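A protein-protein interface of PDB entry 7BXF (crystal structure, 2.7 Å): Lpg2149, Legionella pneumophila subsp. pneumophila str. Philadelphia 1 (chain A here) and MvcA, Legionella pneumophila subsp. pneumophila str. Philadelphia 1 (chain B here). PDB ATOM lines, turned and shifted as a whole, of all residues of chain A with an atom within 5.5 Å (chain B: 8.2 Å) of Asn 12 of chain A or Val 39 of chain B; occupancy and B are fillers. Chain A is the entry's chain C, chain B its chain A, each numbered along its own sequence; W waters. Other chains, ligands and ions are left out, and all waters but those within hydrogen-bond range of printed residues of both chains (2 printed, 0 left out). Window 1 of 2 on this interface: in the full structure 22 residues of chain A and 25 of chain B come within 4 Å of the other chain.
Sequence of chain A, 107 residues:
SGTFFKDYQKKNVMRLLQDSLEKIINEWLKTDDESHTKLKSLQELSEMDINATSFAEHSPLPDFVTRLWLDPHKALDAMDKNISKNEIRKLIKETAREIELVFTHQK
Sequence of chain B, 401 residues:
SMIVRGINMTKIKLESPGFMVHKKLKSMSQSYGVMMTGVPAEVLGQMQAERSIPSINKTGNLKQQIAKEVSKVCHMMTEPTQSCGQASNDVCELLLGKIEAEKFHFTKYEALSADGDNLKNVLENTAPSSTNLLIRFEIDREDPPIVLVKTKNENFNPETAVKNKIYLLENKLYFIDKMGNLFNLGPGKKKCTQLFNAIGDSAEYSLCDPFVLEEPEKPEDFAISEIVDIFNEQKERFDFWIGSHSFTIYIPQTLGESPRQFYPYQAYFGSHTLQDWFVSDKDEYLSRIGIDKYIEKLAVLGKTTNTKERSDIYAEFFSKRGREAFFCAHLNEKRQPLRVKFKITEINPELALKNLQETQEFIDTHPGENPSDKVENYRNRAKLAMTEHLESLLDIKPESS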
ATOM      1  N   ASP A   7      29.428  -4.124  21.071  1.00  0.00           N
ATOM      2  CA  ASP A   7      28.751  -4.076  19.777  1.00  0.00           C
ATOM      3  C   ASP A   7      27.418  -3.346  19.876  1.00  0.00           C
ATOM      4  O   ASP A   7      27.049  -2.582  18.975  1.00  0.00           O
ATOM      5  CB  ASP A   7      28.548  -5.493  19.246  1.00  0.00           C
ATOM      6  CG  ASP A   7      29.852  -6.226  19.059  1.00  0.00           C
ATOM      7  OD1 ASP A   7      30.903  -5.545  19.024  1.00  0.00           O
ATOM      8  OD2 ASP A   7      29.831  -7.472  18.953  1.00  0.00           O
ATOM      9  N   TYR A   8      26.685  -3.578  20.967  1.00  0.00           N
ATOM     10  CA  TYR A   8      25.410  -2.910  21.204  1.00  0.00           C
ATOM     11  C   TYR A   8      25.599  -1.408  21.384  1.00  0.00           C
ATOM     12  O   TYR A   8      24.804  -0.606  20.881  1.00  0.00           O
ATOM     13  CB  TYR A   8      24.756  -3.540  22.433  1.00  0.00           C
ATOM     14  CG  TYR A   8      23.455  -2.939  22.921  1.00  0.00           C
ATOM     15  CD1 TYR A   8      22.287  -3.043  22.176  1.00  0.00           C
ATOM     16  CD2 TYR A   8      23.386  -2.320  24.161  1.00  0.00           C
ATOM     17  CE1 TYR A   8      21.098  -2.517  22.645  1.00  0.00           C
ATOM     18  CE2 TYR A   8      22.202  -1.794  24.635  1.00  0.00           C
ATOM     19  CZ  TYR A   8      21.064  -1.893  23.875  1.00  0.00           C
ATOM     20  OH  TYR A   8      19.889  -1.366  24.357  1.00  0.00           O
ATOM     21  N   GLN A   9      26.652  -1.012  22.099  1.00  0.00           N
ATOM     22  CA  GLN A   9      26.916   0.403  22.323  1.00  0.00           C
ATOM     23  C   GLN A   9      27.344   1.090  21.034  1.00  0.00           C
ATOM     24  O   GLN A   9      26.887   2.200  20.732  1.00  0.00           O
ATOM     25  CB  GLN A   9      27.983   0.546  23.407  1.00  0.00           C
ATOM     26  CG  GLN A   9      28.596   1.919  23.552  1.00  0.00           C
ATOM     27  CD  GLN A   9      29.650   1.938  24.637  1.00  0.00           C
ATOM     28  OE1 GLN A   9      29.433   2.478  25.729  1.00  0.00           O
ATOM     29  NE2 GLN A   9      30.797   1.327  24.353  1.00  0.00           N
ATOM     30  N   LYS A  10      28.226   0.448  20.268  1.00  0.00           N
ATOM     31  CA  LYS A  10      28.636   1.013  18.989  1.00  0.00           C
ATOM     32  C   LYS A  10      27.436   1.184  18.071  1.00  0.00           C
ATOM     33  O   LYS A  10      27.309   2.204  17.387  1.00  0.00           O
ATOM     34  CB  LYS A  10      29.698   0.124  18.341  1.00  0.00           C
ATOM     35  CG  LYS A  10      30.180   0.596  16.980  1.00  0.00           C
ATOM     36  CD  LYS A  10      31.150  -0.398  16.358  1.00  0.00           C
ATOM     37  CE  LYS A  10      31.623   0.085  14.997  1.00  0.00           C
ATOM     38  NZ  LYS A  10      32.677  -0.770  14.386  1.00  0.00           N
ATOM     39  N   LYS A  11      26.525   0.210  18.071  1.00  0.00           N
ATOM     40  CA  LYS A  11      25.317   0.329  17.265  1.00  0.00           C
ATOM     41  C   LYS A  11      24.525   1.569  17.657  1.00  0.00           C
ATOM     42  O   LYS A  11      24.238   2.433  16.819  1.00  0.00           O
ATOM     43  CB  LYS A  11      24.463  -0.929  17.414  1.00  0.00           C
ATOM     44  CG  LYS A  11      23.473  -1.120  16.281  1.00  0.00           C
ATOM     45  CD  LYS A  11      22.818  -2.478  16.355  1.00  0.00           C
ATOM     46  CE  LYS A  11      21.401  -2.360  16.872  1.00  0.00           C
ATOM     47  NZ  LYS A  11      20.434  -2.244  15.750  1.00  0.00           N
ATOM     48  N   ASN A  12      24.182   1.683  18.942  1.00  0.00           N
ATOM     49  CA  ASN A  12      23.343   2.787  19.393  1.00  0.00           C
ATOM     50  C   ASN A  12      24.053   4.130  19.272  1.00  0.00           C
ATOM     51  O   ASN A  12      23.407   5.145  18.997  1.00  0.00           O
ATOM     52  CB  ASN A  12      22.887   2.536  20.827  1.00  0.00           C
ATOM     53  CG  ASN A  12      21.741   1.550  20.901  1.00  0.00           C
ATOM     54  OD1 ASN A  12      20.924   1.470  19.985  1.00  0.00           O
ATOM     55  ND2 ASN A  12      21.671   0.795  21.993  1.00  0.00           N
ATOM     56  N   VAL A  13      25.368   4.160  19.464  1.00  0.00           N
ATOM     57  CA  VAL A  13      26.120   5.380  19.191  1.00  0.00           C
ATOM     58  C   VAL A  13      26.026   5.744  17.712  1.00  0.00           C
ATOM     59  O   VAL A  13      25.834   6.914  17.356  1.00  0.00           O
ATOM     60  CB  VAL A  13      27.578   5.217  19.651  1.00  0.00           C
ATOM     61  CG1 VAL A  13      28.455   6.317  19.058  1.00  0.00           C
ATOM     62  CG2 VAL A  13      27.638   5.242  21.167  1.00  0.00           C
ATOM     63  N   MET A  14      26.145   4.749  16.827  1.00  0.00           N
ATOM     64  CA  MET A  14      26.019   5.023  15.398  1.00  0.00           C
ATOM     65  C   MET A  14      24.610   5.458  15.036  1.00  0.00           C
ATOM     66  O   MET A  14      24.430   6.293  14.141  1.00  0.00           O
ATOM     67  CB  MET A  14      26.416   3.793  14.580  1.00  0.00           C
ATOM     68  CG  MET A  14      27.881   3.408  14.705  1.00  0.00           C
ATOM     69  SD  MET A  14      28.926   4.102  13.428  1.00  0.00           S
ATOM     70  CE  MET A  14      29.189   5.748  14.072  1.00  0.00           C
ATOM     71  N   ARG A  15      23.605   4.911  15.723  1.00  0.00           N
ATOM     72  CA  ARG A  15      22.227   5.294  15.446  1.00  0.00           C
ATOM     73  C   ARG A  15      21.961   6.730  15.883  1.00  0.00           C
ATOM     74  O   ARG A  15      21.339   7.509  15.150  1.00  0.00           O
ATOM     75  CB  ARG A  15      21.269   4.325  16.136  1.00  0.00           C
ATOM     76  CG  ARG A  15      19.806   4.616  15.875  1.00  0.00           C
ATOM     77  CD  ARG A  15      19.427   4.306  14.436  1.00  0.00           C
ATOM     78  NE  ARG A  15      18.482   5.279  13.892  1.00  0.00           N
ATOM     79  CZ  ARG A  15      17.202   5.020  13.648  1.00  0.00           C
ATOM     80  NH1 ARG A  15      16.709   3.814  13.903  1.00  0.00           N
ATOM     81  NH2 ARG A  15      16.416   5.968  13.149  1.00  0.00           N
ATOM     82  N   LEU A  16      22.427   7.101  17.075  1.00  0.00           N
ATOM     83  CA  LEU A  16      22.237   8.472  17.535  1.00  0.00           C
ATOM     84  C   LEU A  16      22.903   9.465  16.586  1.00  0.00           C
ATOM     85  O   LEU A  16      22.360  10.545  16.327  1.00  0.00           O
ATOM     86  CB  LEU A  16      22.772   8.619  18.960  1.00  0.00           C
ATOM     87  CG  LEU A  16      22.625  10.008  19.584  1.00  0.00           C
ATOM     88  CD1 LEU A  16      21.165  10.439  19.558  1.00  0.00           C
ATOM     89  CD2 LEU A  16      23.178  10.017  21.002  1.00  0.00           C
ATOM     90  N   LEU A  17      24.069   9.104  16.040  1.00  0.00           N
ATOM     91  CA  LEU A  17      24.743   9.961  15.064  1.00  0.00           C
ATOM     92  C   LEU A  17      23.892  10.151  13.815  1.00  0.00           C
ATOM     93  O   LEU A  17      23.647  11.284  13.382  1.00  0.00           O
ATOM     94  CB  LEU A  17      26.108   9.372  14.704  1.00  0.00           C
ATOM     95  CG  LEU A  17      27.020  10.183  13.781  1.00  0.00           C
ATOM     96  CD1 LEU A  17      27.328  11.539  14.370  1.00  0.00           C
ATOM     97  CD2 LEU A  17      28.300   9.429  13.528  1.00  0.00           C
ATOM     98  N   VAL B  34      17.161   5.966  29.059  1.00  0.00           N
ATOM     99  CA  VAL B  34      18.026   6.129  27.888  1.00  0.00           C
ATOM    100  C   VAL B  34      19.405   5.516  28.083  1.00  0.00           C
ATOM    101  O   VAL B  34      20.099   5.244  27.099  1.00  0.00           O
ATOM    102  CB  VAL B  34      18.161   7.629  27.529  1.00  0.00           C
ATOM    103  CG1 VAL B  34      19.041   8.344  28.551  1.00  0.00           C
ATOM    104  CG2 VAL B  34      18.708   7.807  26.109  1.00  0.00           C
ATOM    105  N   MET B  35      19.794   5.287  29.331  1.00  0.00           N
ATOM    106  CA  MET B  35      21.117   4.724  29.682  1.00  0.00           C
ATOM    107  C   MET B  35      21.202   3.290  29.155  1.00  0.00           C
ATOM    108  O   MET B  35      22.281   2.833  28.869  1.00  0.00           O
ATOM    109  CB  MET B  35      21.288   4.726  31.198  1.00  0.00           C
ATOM    110  CG  MET B  35      21.656   6.051  31.759  1.00  0.00           C
ATOM    111  SD  MET B  35      21.558   6.175  33.537  1.00  0.00           S
ATOM    112  CE  MET B  35      23.160   5.612  34.065  1.00  0.00           C
ATOM    113  N   MET B  36      20.056   2.654  28.985  1.00  0.00           N
ATOM    114  CA  MET B  36      19.933   1.262  28.520  1.00  0.00           C
ATOM    115  C   MET B  36      20.327   1.134  27.054  1.00  0.00           C
ATOM    116  O   MET B  36      20.456   0.018  26.594  1.00  0.00           O
ATOM    117  CB  MET B  36      18.499   0.791  28.718  1.00  0.00           C
ATOM    118  CG  MET B  36      18.316  -0.126  29.881  1.00  0.00           C
ATOM    119  SD  MET B  36      17.248  -1.482  29.400  1.00  0.00           S
ATOM    120  CE  MET B  36      16.174  -0.694  28.214  1.00  0.00           C
ATOM    121  N   THR B  37      20.443   2.234  26.329  1.00  0.00           N
ATOM    122  CA  THR B  37      20.970   2.174  24.974  1.00  0.00           C
ATOM    123  C   THR B  37      22.460   1.868  24.966  1.00  0.00           C
ATOM    124  O   THR B  37      22.976   1.382  23.955  1.00  0.00           O
ATOM    125  CB  THR B  37      20.703   3.490  24.242  1.00  0.00           C
ATOM    126  OG1 THR B  37      21.478   4.533  24.843  1.00  0.00           O
ATOM    127  CG2 THR B  37      19.224   3.855  24.329  1.00  0.00           C
ATOM    128  N   GLY B  38      23.150   2.116  26.081  1.00  0.00           N
ATOM    129  CA  GLY B  38      24.582   1.948  26.168  1.00  0.00           C
ATOM    130  C   GLY B  38      25.394   3.180  25.819  1.00  0.00           C
ATOM    131  O   GLY B  38      26.616   3.172  26.018  1.00  0.00           O
ATOM    132  N   VAL B  39      24.758   4.235  25.316  1.00  0.00           N
ATOM    133  CA  VAL B  39      25.447   5.433  24.846  1.00  0.00           C
ATOM    134  C   VAL B  39      26.137   6.120  26.021  1.00  0.00           C
ATOM    135  O   VAL B  39      25.482   6.442  27.024  1.00  0.00           O
ATOM    136  CB  VAL B  39      24.466   6.381  24.135  1.00  0.00           C
ATOM    137  CG1 VAL B  39      25.159   7.690  23.727  1.00  0.00           C
ATOM    138  CG2 VAL B  39      23.853   5.689  22.921  1.00  0.00           C
ATOM    139  N   PRO B  40      27.450   6.346  25.955  1.00  0.00           N
ATOM    140  CA  PRO B  40      28.112   7.114  27.015  1.00  0.00           C
ATOM    141  C   PRO B  40      27.502   8.505  27.120  1.00  0.00           C
ATOM    142  O   PRO B  40      27.134   9.118  26.114  1.00  0.00           O
ATOM    143  CB  PRO B  40      29.578   7.166  26.559  1.00  0.00           C
ATOM    144  CG  PRO B  40      29.730   6.011  25.603  1.00  0.00           C
ATOM    145  CD  PRO B  40      28.397   5.908  24.910  1.00  0.00           C
ATOM    146  N   ALA B  41      27.378   8.997  28.354  1.00  0.00           N
ATOM    147  CA  ALA B  41      26.816  10.326  28.554  1.00  0.00           C
ATOM    148  C   ALA B  41      27.613  11.375  27.788  1.00  0.00           C
ATOM    149  O   ALA B  41      27.039  12.323  27.239  1.00  0.00           O
ATOM    150  CB  ALA B  41      26.767  10.662  30.046  1.00  0.00           C
ATOM    151  N   GLU B  42      28.935  11.205  27.718  1.00  0.00           N
ATOM    152  CA  GLU B  42      29.771  12.157  26.990  1.00  0.00           C
ATOM    153  C   GLU B  42      29.410  12.204  25.513  1.00  0.00           C
ATOM    154  O   GLU B  42      29.358  13.284  24.914  1.00  0.00           O
ATOM    155  CB  GLU B  42      31.242  11.787  27.139  1.00  0.00           C
ATOM    156  CG  GLU B  42      31.703  11.667  28.534  1.00  0.00           C
ATOM    157  CD  GLU B  42      32.591  12.817  28.931  1.00  0.00           C
ATOM    158  OE1 GLU B  42      33.609  12.574  29.612  1.00  0.00           O
ATOM    159  OE2 GLU B  42      32.263  13.965  28.564  1.00  0.00           O
ATOM    160  N   VAL B  43      29.194  11.037  24.906  1.00  0.00           N
ATOM    161  CA  VAL B  43      28.783  10.974  23.506  1.00  0.00           C
ATOM    162  C   VAL B  43      27.438  11.667  23.304  1.00  0.00           C
ATOM    163  O   VAL B  43      27.235  12.389  22.319  1.00  0.00           O
ATOM    164  CB  VAL B  43      28.740   9.503  23.043  1.00  0.00           C
ATOM    165  CG1 VAL B  43      28.105   9.387  21.681  1.00  0.00           C
ATOM    166  CG2 VAL B  43      30.132   8.907  23.033  1.00  0.00           C
ATOM    167  N   LEU B  44      26.499  11.462  24.231  1.00  0.00           N
ATOM    168  CA  LEU B  44      25.146  11.975  24.033  1.00  0.00           C
ATOM    169  C   LEU B  44      25.094  13.489  24.184  1.00  0.00           C
ATOM    170  O   LEU B  44      24.395  14.173  23.423  1.00  0.00           O
ATOM    171  CB  LEU B  44      24.182  11.298  25.008  1.00  0.00           C
ATOM    172  CG  LEU B  44      22.830  11.986  25.194  1.00  0.00           C
ATOM    173  CD1 LEU B  44      21.967  11.768  23.956  1.00  0.00           C
ATOM    174  CD2 LEU B  44      22.119  11.511  26.458  1.00  0.00           C
ATOM    175  N   GLY B  45      25.821  14.036  25.160  1.00  0.00           N
ATOM    176  CA  GLY B  45      25.870  15.481  25.305  1.00  0.00           C
ATOM    177  C   GLY B  45      26.572  16.157  24.143  1.00  0.00           C
ATOM    178  O   GLY B  45      26.121  17.194  23.653  1.00  0.00           O
ATOM    179  N   MET B  47      26.736  15.204  21.091  1.00  0.00           N
ATOM    180  CA  MET B  47      25.821  15.117  19.921  1.00  0.00           C
ATOM    181  C   MET B  47      24.737  16.188  20.059  1.00  0.00           C
ATOM    182  O   MET B  47      24.534  16.950  19.092  1.00  0.00           O
ATOM    183  CB  MET B  47      25.161  13.736  19.847  1.00  0.00           C
ATOM    184  CG  MET B  47      25.381  13.031  18.523  1.00  0.00           C
ATOM    185  SD  MET B  47      25.467  11.231  18.700  1.00  0.00           S
ATOM    186  CE  MET B  47      27.216  10.957  18.418  1.00  0.00           C
ATOM    187  N   GLY B  85      10.872   2.285  16.882  1.00  0.00           N
ATOM    188  CA  GLY B  85      11.870   1.404  16.298  1.00  0.00           C
ATOM    189  C   GLY B  85      13.096   1.234  17.174  1.00  0.00           C
ATOM    190  O   GLY B  85      13.645   0.134  17.275  1.00  0.00           O
ATOM    191  N   GLN B  86      13.544   2.315  17.819  1.00  0.00           N
ATOM    192  CA  GLN B  86      14.685   2.215  18.722  1.00  0.00           C
ATOM    193  C   GLN B  86      14.368   1.331  19.925  1.00  0.00           C
ATOM    194  O   GLN B  86      15.220   0.551  20.372  1.00  0.00           O
ATOM    195  CB  GLN B  86      15.122   3.607  19.177  1.00  0.00           C
ATOM    196  CG  GLN B  86      16.353   3.604  20.067  1.00  0.00           C
ATOM    197  CD  GLN B  86      17.597   3.172  19.328  1.00  0.00           C
ATOM    198  OE1 GLN B  86      17.686   3.320  18.108  1.00  0.00           O
ATOM    199  NE2 GLN B  86      18.564   2.628  20.058  1.00  0.00           N
ATOM    200  N   ALA B  87      13.149   1.437  20.467  1.00  0.00           N
ATOM    201  CA  ALA B  87      12.752   0.562  21.567  1.00  0.00           C
ATOM    202  C   ALA B  87      12.683  -0.890  21.105  1.00  0.00           C
ATOM    203  O   ALA B  87      13.277  -1.780  21.726  1.00  0.00           O
ATOM    204  CB  ALA B  87      11.414   1.019  22.146  1.00  0.00           C
ATOM    205  N   ASN B  89      14.175  -2.163  18.575  1.00  0.00           N
ATOM    206  CA  ASN B  89      15.520  -2.621  18.234  1.00  0.00           C
ATOM    207  C   ASN B  89      16.326  -2.961  19.478  1.00  0.00           C
ATOM    208  O   ASN B  89      17.023  -3.980  19.504  1.00  0.00           O
ATOM    209  CB  ASN B  89      16.243  -1.569  17.394  1.00  0.00           C
ATOM    210  CG  ASN B  89      15.849  -1.633  15.931  1.00  0.00           C
ATOM    211  OD1 ASN B  89      15.012  -2.450  15.538  1.00  0.00           O
ATOM    212  ND2 ASN B  89      16.442  -0.769  15.120  1.00  0.00           N
ATOM    213  N   ASP B  90      16.245  -2.118  20.518  1.00  0.00           N
ATOM    214  CA  ASP B  90      16.921  -2.415  21.779  1.00  0.00           C
ATOM    215  C   ASP B  90      16.462  -3.754  22.354  1.00  0.00           C
ATOM    216  O   ASP B  90      17.279  -4.534  22.856  1.00  0.00           O
ATOM    217  CB  ASP B  90      16.665  -1.293  22.791  1.00  0.00           C
ATOM    218  CG  ASP B  90      17.465  -0.027  22.496  1.00  0.00           C
ATOM    219  OD1 ASP B  90      18.393  -0.080  21.657  1.00  0.00           O
ATOM    220  OD2 ASP B  90      17.141   1.025  23.101  1.00  0.00           O
ATOM    221  N   VAL B  91      15.161  -4.043  22.275  1.00  0.00           N
ATOM    222  CA  VAL B  91      14.626  -5.273  22.854  1.00  0.00           C
ATOM    223  C   VAL B  91      15.160  -6.490  22.112  1.00  0.00           C
ATOM    224  O   VAL B  91      15.632  -7.456  22.724  1.00  0.00           O
ATOM    225  CB  VAL B  91      13.087  -5.248  22.850  1.00  0.00           C
ATOM    226  CG1 VAL B  91      12.535  -6.629  23.172  1.00  0.00           C
ATOM    227  CG2 VAL B  91      12.562  -4.214  23.839  1.00  0.00           C
ATOM    228  N   GLU B  93      17.833  -6.681  20.225  1.00  0.00           N
ATOM    229  CA  GLU B  93      19.271  -6.769  20.452  1.00  0.00           C
ATOM    230  C   GLU B  93      19.582  -7.398  21.805  1.00  0.00           C
ATOM    231  O   GLU B  93      20.487  -8.232  21.914  1.00  0.00           O
ATOM    232  CB  GLU B  93      19.903  -5.382  20.354  1.00  0.00           C
ATOM    233  CG  GLU B  93      20.194  -4.927  18.943  1.00  0.00           C
ATOM    234  CD  GLU B  93      21.314  -5.714  18.291  1.00  0.00           C
ATOM    235  OE1 GLU B  93      22.140  -6.300  19.023  1.00  0.00           O
ATOM    236  OE2 GLU B  93      21.371  -5.741  17.046  1.00  0.00           O
ATOM    237  N   LEU B  94      18.835  -7.019  22.848  1.00  0.00           N
ATOM    238  CA  LEU B  94      19.134  -7.499  24.194  1.00  0.00           C
ATOM    239  C   LEU B  94      18.803  -8.983  24.346  1.00  0.00           C
ATOM    240  O   LEU B  94      19.610  -9.761  24.871  1.00  0.00           O
ATOM    241  CB  LEU B  94      18.379  -6.657  25.226  1.00  0.00           C
ATOM    242  CG  LEU B  94      18.996  -5.294  25.579  1.00  0.00           C
ATOM    243  CD1 LEU B  94      18.002  -4.366  26.282  1.00  0.00           C
ATOM    244  CD2 LEU B  94      20.240  -5.473  26.428  1.00  0.00           C
ATOM    245  N   THR B 359      25.012  -4.917  30.240  1.00  0.00           N
ATOM    246  CA  THR B 359      24.442  -3.573  30.159  1.00  0.00           C
ATOM    247  C   THR B 359      24.392  -2.904  31.531  1.00  0.00           C
ATOM    248  O   THR B 359      24.729  -1.720  31.657  1.00  0.00           O
ATOM    249  CB  THR B 359      23.045  -3.622  29.526  1.00  0.00           C
ATOM    250  OG1 THR B 359      23.106  -4.299  28.266  1.00  0.00           O
ATOM    251  CG2 THR B 359      22.513  -2.214  29.287  1.00  0.00           C
ATOM    252  N   PHE B 362      27.763  -1.620  32.583  1.00  0.00           N
ATOM    253  CA  PHE B 362      27.971  -0.255  32.101  1.00  0.00           C
ATOM    254  C   PHE B 362      27.236   0.747  32.976  1.00  0.00           C
ATOM    255  O   PHE B 362      27.783   1.802  33.320  1.00  0.00           O
ATOM    256  CB  PHE B 362      27.504  -0.136  30.645  1.00  0.00           C
ATOM    257  CG  PHE B 362      27.332   1.294  30.149  1.00  0.00           C
ATOM    258  CD1 PHE B 362      28.435   2.115  29.927  1.00  0.00           C
ATOM    259  CD2 PHE B 362      26.066   1.800  29.871  1.00  0.00           C
ATOM    260  CE1 PHE B 362      28.274   3.426  29.457  1.00  0.00           C
ATOM    261  CE2 PHE B 362      25.894   3.112  29.403  1.00  0.00           C
ATOM    262  CZ  PHE B 362      27.002   3.924  29.195  1.00  0.00           C
ATOM    263  N   HIS B 366      28.506   4.365  36.630  1.00  0.00           N
ATOM    264  CA  HIS B 366      28.152   5.731  36.969  1.00  0.00           C
ATOM    265  C   HIS B 366      27.982   5.841  38.475  1.00  0.00           C
ATOM    266  O   HIS B 366      27.201   5.073  39.056  1.00  0.00           O
ATOM    267  CB  HIS B 366      26.881   6.133  36.251  1.00  0.00           C
ATOM    268  CG  HIS B 366      26.983   6.007  34.764  1.00  0.00           C
ATOM    269  ND1 HIS B 366      26.948   4.789  34.119  1.00  0.00           N
ATOM    270  CD2 HIS B 366      27.154   6.940  33.798  1.00  0.00           C
ATOM    271  CE1 HIS B 366      27.083   4.979  32.818  1.00  0.00           C
ATOM    272  NE2 HIS B 366      27.207   6.274  32.598  1.00  0.00           N
ATOM    273  N   TYR B 378      24.407  10.484  35.088  1.00  0.00           N
ATOM    274  CA  TYR B 378      24.384  10.461  33.630  1.00  0.00           C
ATOM    275  C   TYR B 378      23.989  11.824  33.066  1.00  0.00           C
ATOM    276  O   TYR B 378      24.649  12.345  32.162  1.00  0.00           O
ATOM    277  CB  TYR B 378      23.419   9.371  33.163  1.00  0.00           C
ATOM    278  CG  TYR B 378      23.494   9.006  31.698  1.00  0.00           C
ATOM    279  CD1 TYR B 378      24.437   8.100  31.234  1.00  0.00           C
ATOM    280  CD2 TYR B 378      22.588   9.534  30.789  1.00  0.00           C
ATOM    281  CE1 TYR B 378      24.495   7.760  29.891  1.00  0.00           C
ATOM    282  CE2 TYR B 378      22.634   9.200  29.450  1.00  0.00           C
ATOM    283  CZ  TYR B 378      23.588   8.318  29.004  1.00  0.00           C
ATOM    284  OH  TYR B 378      23.626   7.999  27.666  1.00  0.00           O
ATOM    285  N   ALA B 382      26.368  14.267  31.071  1.00  0.00           N
ATOM    286  CA  ALA B 382      26.012  14.606  29.673  1.00  0.00           C
ATOM    287  C   ALA B 382      25.950  16.127  29.485  1.00  0.00           C
ATOM    288  O   ALA B 382      26.467  16.615  28.460  1.00  0.00           O
ATOM    289  CB  ALA B 382      24.696  13.957  29.320  1.00  0.00           C
HETATM  290  O   HOH W   1      24.668  -5.299  18.736  1.00  0.00           O
HETATM  291  O   HOH W   2      19.683  -0.615  19.063  1.00  0.00           O
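Water W2 bridges the side-chain amide oxygen (OD1) of Asn 12 of chain A (2.6 Å) and the side-chain carboxylate (OD1) of Asp 90 of chain B (2.9 Å).
Water W1 lies within hydrogen-bond range of the side-chain carboxylate (OE1) of Glu 93 of chain B and the backbone NH (N) of Tyr 8 of chain A.
O of Val 34 of chain B sits at hydrogen-bond distance from OG1 of Thr 37 of chain B.
The side-chain hydroxyl of Tyr 378 of chain B is in hydrogen-bond range of the backbone carbonyl oxygen of Val 39 of chain B, 2.5 Å away.
The side-chain amide nitrogen of Gln 86 of chain B is in hydrogen-bond range of the side-chain carboxylate of Asp 90 of chain B, 3.1 Å away.
Of chain B, only Thr 37, Val 39, Gln 86 and Asp 90 come within 4 Å of Asn 12 of chain A.
Of chain A, only Asn 12 (3.9 Å) comes within 4 Å of Val 39 of chain B.
Of the printed residues of chain A, Asp 90 of chain B touches Tyr 8 and Asn 12.
Of the printed residues of chain B, Leu 16 of chain A touches Leu 44 (3.6 Å) and Met 47 (3.2 Å).
Leu 94 of chain B touches none of the printed residues of chain A.
His 366 of chain B touches none of the printed residues of chain A.
The nearest residue of chain B that does not touch Asn 12 of chain A is Gly 38 of chain B (4.5 Å).
The nearest printed residue of chain A that does not touch Val 39 of chain B is Val 13 of chain A (4.1 Å).
The nearest printed residue of chain A that does not touch Thr 37 of chain B is Gln 9 of chain A (4.4 Å).
The side-chain hydroxyl of Tyr 8 of chain A sits at hydrogen-bond distance from the backbone carbonyl oxygen of Met 36 of chain B.
The backbone carbonyl oxygen (O) of Thr 37 of chain B is in hydrogen-bond range of the side-chain amide nitrogen (ND2) of Asn 12 of chain A.
The backbone carbonyl oxygen of Gly 38 of chain B sits close to the side-chain amide oxygen of Gln 9 of chain A, 2.9 Å away.
The backbone NH (N) of Leu 17 of chain A lies within hydrogen-bond range of the side-chain sulfur (SD) of Met 47 of chain B (3.7 Å).
The side-chain amide nitrogen (NE2) of Gln 86 of chain B sits at hydrogen-bond distance from the side-chain amide oxygen (OD1) of Asn 12 of chain A.
OH of Tyr 8 of chain A sits close to OD1 of Asp 90 of chain B, at 3.3 Å.
The side-chain amide oxygen (OD1) of Asn 12 of chain A lies close to the side-chain carboxylate (OD1) of Asp 90 of chain B (3.4 Å).
OE2 of Glu 93 of chain B lies within salt-bridge range of NZ of Lys 11 of chain A (3.8 Å).
Of the 11 printed residues of chain A, 8 touch a printed residue of chain B.
Of the 26 printed residues of chain B, 10 touch a printed residue of chain A.
Hydrophobic or aromatic side chains of chain B within 4 Å of the printed part of chain A: Val 39, Pro 40, Leu 44 and Met 47.
Among the printed residues, 16 pairs touch across the chains.
Among the printed residues, Asp or Glu carboxylates within 4 Å of a Lys or Arg side-chain nitrogen of the other chain: Lys 11 of chain A with Glu 93 of chain B (3.8 Å).
Glu 93 of chain B touches Tyr 8 of chain A.
OE1 of Gln 9 of chain A touches CG of Pro 40 of chain B (3.5 Å).
CB of Asn 12 of chain A touches CG2 of Val 39 of chain B, 3.9 Å away.
Arg 15 of chain A touches Gln 86 of chain B (CG to OE1, 3.3 Å).
Leu 16 of chain A touches Leu 44 of chain B (CD2 to CD1, 3.6 Å).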
